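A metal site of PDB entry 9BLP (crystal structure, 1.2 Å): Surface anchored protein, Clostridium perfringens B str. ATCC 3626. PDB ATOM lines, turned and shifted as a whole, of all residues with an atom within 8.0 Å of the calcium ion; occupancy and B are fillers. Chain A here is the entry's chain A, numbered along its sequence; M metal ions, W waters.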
ATOM      1  N   ILE A 125      23.146  28.406 -21.320  1.00  0.00           N
ATOM      2  CA  ILE A 125      24.128  27.350 -20.949  1.00  0.00           C
ATOM      3  C   ILE A 125      24.447  26.523 -22.188  1.00  0.00           C
ATOM      4  O   ILE A 125      23.522  26.107 -22.910  1.00  0.00           O
ATOM      5  CB  ILE A 125      23.625  26.480 -19.792  1.00  0.00           C
ATOM      6  CG1 ILE A 125      23.316  27.313 -18.544  1.00  0.00           C
ATOM      7  CG2 ILE A 125      24.638  25.384 -19.485  1.00  0.00           C
ATOM      8  CD1 ILE A 125      22.615  26.554 -17.451  1.00  0.00           C
ATOM      9  N   ASP A 126      25.730  26.262 -22.402  1.00  0.00           N
ATOM     10  CA  ASP A 126      26.244  25.298 -23.396  1.00  0.00           C
ATOM     11  C   ASP A 126      26.462  23.969 -22.670  1.00  0.00           C
ATOM     12  O   ASP A 126      27.325  23.925 -21.769  1.00  0.00           O
ATOM     13  CB  ASP A 126      27.558  25.802 -23.981  1.00  0.00           C
ATOM     14  CG  ASP A 126      28.211  24.810 -24.913  1.00  0.00           C
ATOM     15  OD1 ASP A 126      27.480  23.963 -25.469  1.00  0.00           O
ATOM     16  OD2 ASP A 126      29.441  24.910 -25.090  1.00  0.00           O
ATOM     17  N   THR A 127      25.716  22.942 -23.043  1.00  0.00           N
ATOM     18  CA  THR A 127      25.780  21.615 -22.368  1.00  0.00           C
ATOM     19  C   THR A 127      26.523  20.571 -23.215  1.00  0.00           C
ATOM     20  O   THR A 127      26.608  19.431 -22.746  1.00  0.00           O
ATOM     21  CB  THR A 127      24.388  21.095 -21.999  1.00  0.00           C
ATOM     22  OG1 THR A 127      23.659  20.840 -23.204  1.00  0.00           O
ATOM     23  CG2 THR A 127      23.612  22.040 -21.118  1.00  0.00           C
ATOM     24  N   ASP A 128      27.027  20.920 -24.395  1.00  0.00           N
ATOM     25  CA  ASP A 128      27.657  19.910 -25.291  1.00  0.00           C
ATOM     26  C   ASP A 128      28.949  20.454 -25.923  1.00  0.00           C
ATOM     27  O   ASP A 128      29.356  19.911 -26.966  1.00  0.00           O
ATOM     28  CB  ASP A 128      26.658  19.393 -26.325  1.00  0.00           C
ATOM     29  CG  ASP A 128      26.020  20.443 -27.198  1.00  0.00           C
ATOM     30  OD1 ASP A 128      26.429  21.625 -27.122  1.00  0.00           O
ATOM     31  OD2 ASP A 128      25.109  20.077 -27.968  1.00  0.00           O
ATOM     32  N   LYS A 129      29.592  21.437 -25.293  1.00  0.00           N
ATOM     33  CA  LYS A 129      30.974  21.867 -25.602  1.00  0.00           C
ATOM     34  C   LYS A 129      31.083  22.380 -27.044  1.00  0.00           C
ATOM     35  O   LYS A 129      32.182  22.306 -27.604  1.00  0.00           O
ATOM     36  CB  LYS A 129      31.960  20.726 -25.351  1.00  0.00           C
ATOM     37  CG  LYS A 129      31.960  20.177 -23.937  1.00  0.00           C
ATOM     38  CD  LYS A 129      33.033  19.132 -23.695  1.00  0.00           C
ATOM     39  CE  LYS A 129      33.188  18.795 -22.236  1.00  0.00           C
ATOM     40  NZ  LYS A 129      31.914  18.324 -21.626  1.00  0.00           N
ATOM     41  N   ASP A 130      30.022  22.927 -27.623  1.00  0.00           N
ATOM     42  CA  ASP A 130      30.114  23.534 -28.982  1.00  0.00           C
ATOM     43  C   ASP A 130      30.107  25.065 -28.899  1.00  0.00           C
ATOM     44  O   ASP A 130      30.139  25.699 -29.955  1.00  0.00           O
ATOM     45  CB  ASP A 130      29.057  22.992 -29.934  1.00  0.00           C
ATOM     46  CG  ASP A 130      27.658  23.498 -29.653  1.00  0.00           C
ATOM     47  OD1 ASP A 130      27.466  24.165 -28.608  1.00  0.00           O
ATOM     48  OD2 ASP A 130      26.761  23.219 -30.474  1.00  0.00           O
ATOM     49  N   TYR A 131      30.109  25.630 -27.687  1.00  0.00           N
ATOM     50  CA  TYR A 131      30.175  27.101 -27.438  1.00  0.00           C
ATOM     51  C   TYR A 131      28.983  27.794 -28.109  1.00  0.00           C
ATOM     52  O   TYR A 131      29.070  28.988 -28.424  1.00  0.00           O
ATOM     53  CB  TYR A 131      31.568  27.606 -27.833  1.00  0.00           C
ATOM     54  CG  TYR A 131      32.601  27.145 -26.830  1.00  0.00           C
ATOM     55  CD1 TYR A 131      33.072  25.841 -26.838  1.00  0.00           C
ATOM     56  CD2 TYR A 131      33.041  27.991 -25.816  1.00  0.00           C
ATOM     57  CE1 TYR A 131      33.967  25.396 -25.878  1.00  0.00           C
ATOM     58  CE2 TYR A 131      33.942  27.553 -24.857  1.00  0.00           C
ATOM     59  CZ  TYR A 131      34.397  26.249 -24.891  1.00  0.00           C
ATOM     60  OH  TYR A 131      35.294  25.811 -23.963  1.00  0.00           O
ATOM     61  N   ASN A 132      27.899  27.041 -28.281  1.00  0.00           N
ATOM     62  CA  ASN A 132      26.560  27.563 -28.641  1.00  0.00           C
ATOM     63  C   ASN A 132      25.606  27.296 -27.482  1.00  0.00           C
ATOM     64  O   ASN A 132      25.632  26.181 -26.930  1.00  0.00           O
ATOM     65  CB  ASN A 132      26.029  26.935 -29.931  1.00  0.00           C
ATOM     66  CG  ASN A 132      26.672  27.502 -31.178  1.00  0.00           C
ATOM     67  OD1 ASN A 132      26.017  28.178 -31.967  1.00  0.00           O
ATOM     68  ND2 ASN A 132      27.949  27.236 -31.369  1.00  0.00           N
ATOM     69  N   LEU A 133      24.798  28.272 -27.128  1.00  0.00           N
ATOM     70  CA  LEU A 133      23.886  28.162 -25.970  1.00  0.00           C
ATOM     71  C   LEU A 133      22.687  27.308 -26.351  1.00  0.00           C
ATOM     72  O   LEU A 133      22.066  27.536 -27.410  1.00  0.00           O
ATOM     73  CB  LEU A 133      23.471  29.561 -25.524  1.00  0.00           C
ATOM     74  CG  LEU A 133      24.639  30.487 -25.203  1.00  0.00           C
ATOM     75  CD1 LEU A 133      24.142  31.880 -24.869  1.00  0.00           C
ATOM     76  CD2 LEU A 133      25.484  29.925 -24.065  1.00  0.00           C
ATOM     77  N   ASP A 134      22.354  26.325 -25.503  1.00  0.00           N
ATOM     78  CA  ASP A 134      21.316  25.322 -25.858  1.00  0.00           C
ATOM     79  C   ASP A 134      20.332  25.051 -24.721  1.00  0.00           C
ATOM     80  O   ASP A 134      19.311  24.394 -24.993  1.00  0.00           O
ATOM     81  CB  ASP A 134      21.983  24.029 -26.331  1.00  0.00           C
ATOM     82  CG  ASP A 134      22.890  23.415 -25.283  1.00  0.00           C
ATOM     83  OD1 ASP A 134      22.356  22.887 -24.297  1.00  0.00           O
ATOM     84  OD2 ASP A 134      24.120  23.464 -25.460  1.00  0.00           O
ATOM     85  N   THR A 135      20.611  25.516 -23.495  1.00  0.00           N
ATOM     86  CA  THR A 135      19.793  25.157 -22.309  1.00  0.00           C
ATOM     87  C   THR A 135      19.547  26.412 -21.457  1.00  0.00           C
ATOM     88  O   THR A 135      20.465  27.253 -21.334  1.00  0.00           O
ATOM     89  CB  THR A 135      20.451  24.022 -21.529  1.00  0.00           C
ATOM     90  OG1 THR A 135      20.466  22.871 -22.368  1.00  0.00           O
ATOM     91  CG2 THR A 135      19.737  23.666 -20.239  1.00  0.00           C
HETATM   92 CA    CA M   1      25.785  23.838 -27.058  1.00  0.00          CA
HETATM   93  O   HOH W   1      24.391  23.691 -28.951  1.00  0.00           O
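Of the 11 residues printed, 5 come within 4 Å of the calcium ion. The nearest printed residue that does not touch the calcium ion is Thr 127 (4.1 Å).
The side-chain carboxylate of Asp 126 lies within hydrogen-bond range of the backbone NH of Tyr 131 (2.8 Å). The backbone NH of Lys 129 lies close to the side-chain carboxylate of Asp 126. The side-chain carboxylate of Asp 134 is in hydrogen-bond range of the side-chain hydroxyl of Thr 127 (2.7 Å). The backbone carbonyl oxygen (O) of Ile 125 sits at hydrogen-bond distance from the backbone NH (N) of Asp 134 (2.9 Å). OD1 of Asp 134 lies within hydrogen-bond range of OG1 of Thr 135, 2.7 Å away.
The calcium ion is bound by OD1 of Asp 128, at 2.3 Å. OD1 of Asp 130 is bound to the calcium ion (2.3 Å). OD1 of Asp 126 binds the calcium ion (2.3 Å). OD2 of Asp 134 binds the calcium ion (2.3 Å). The calcium ion is bound by the backbone carbonyl oxygen (O) of Asn 132 (2.4 Å). Water W1 binds the calcium ion, 2.4 Å away. The calcium ion has six donor atoms within binding distance.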
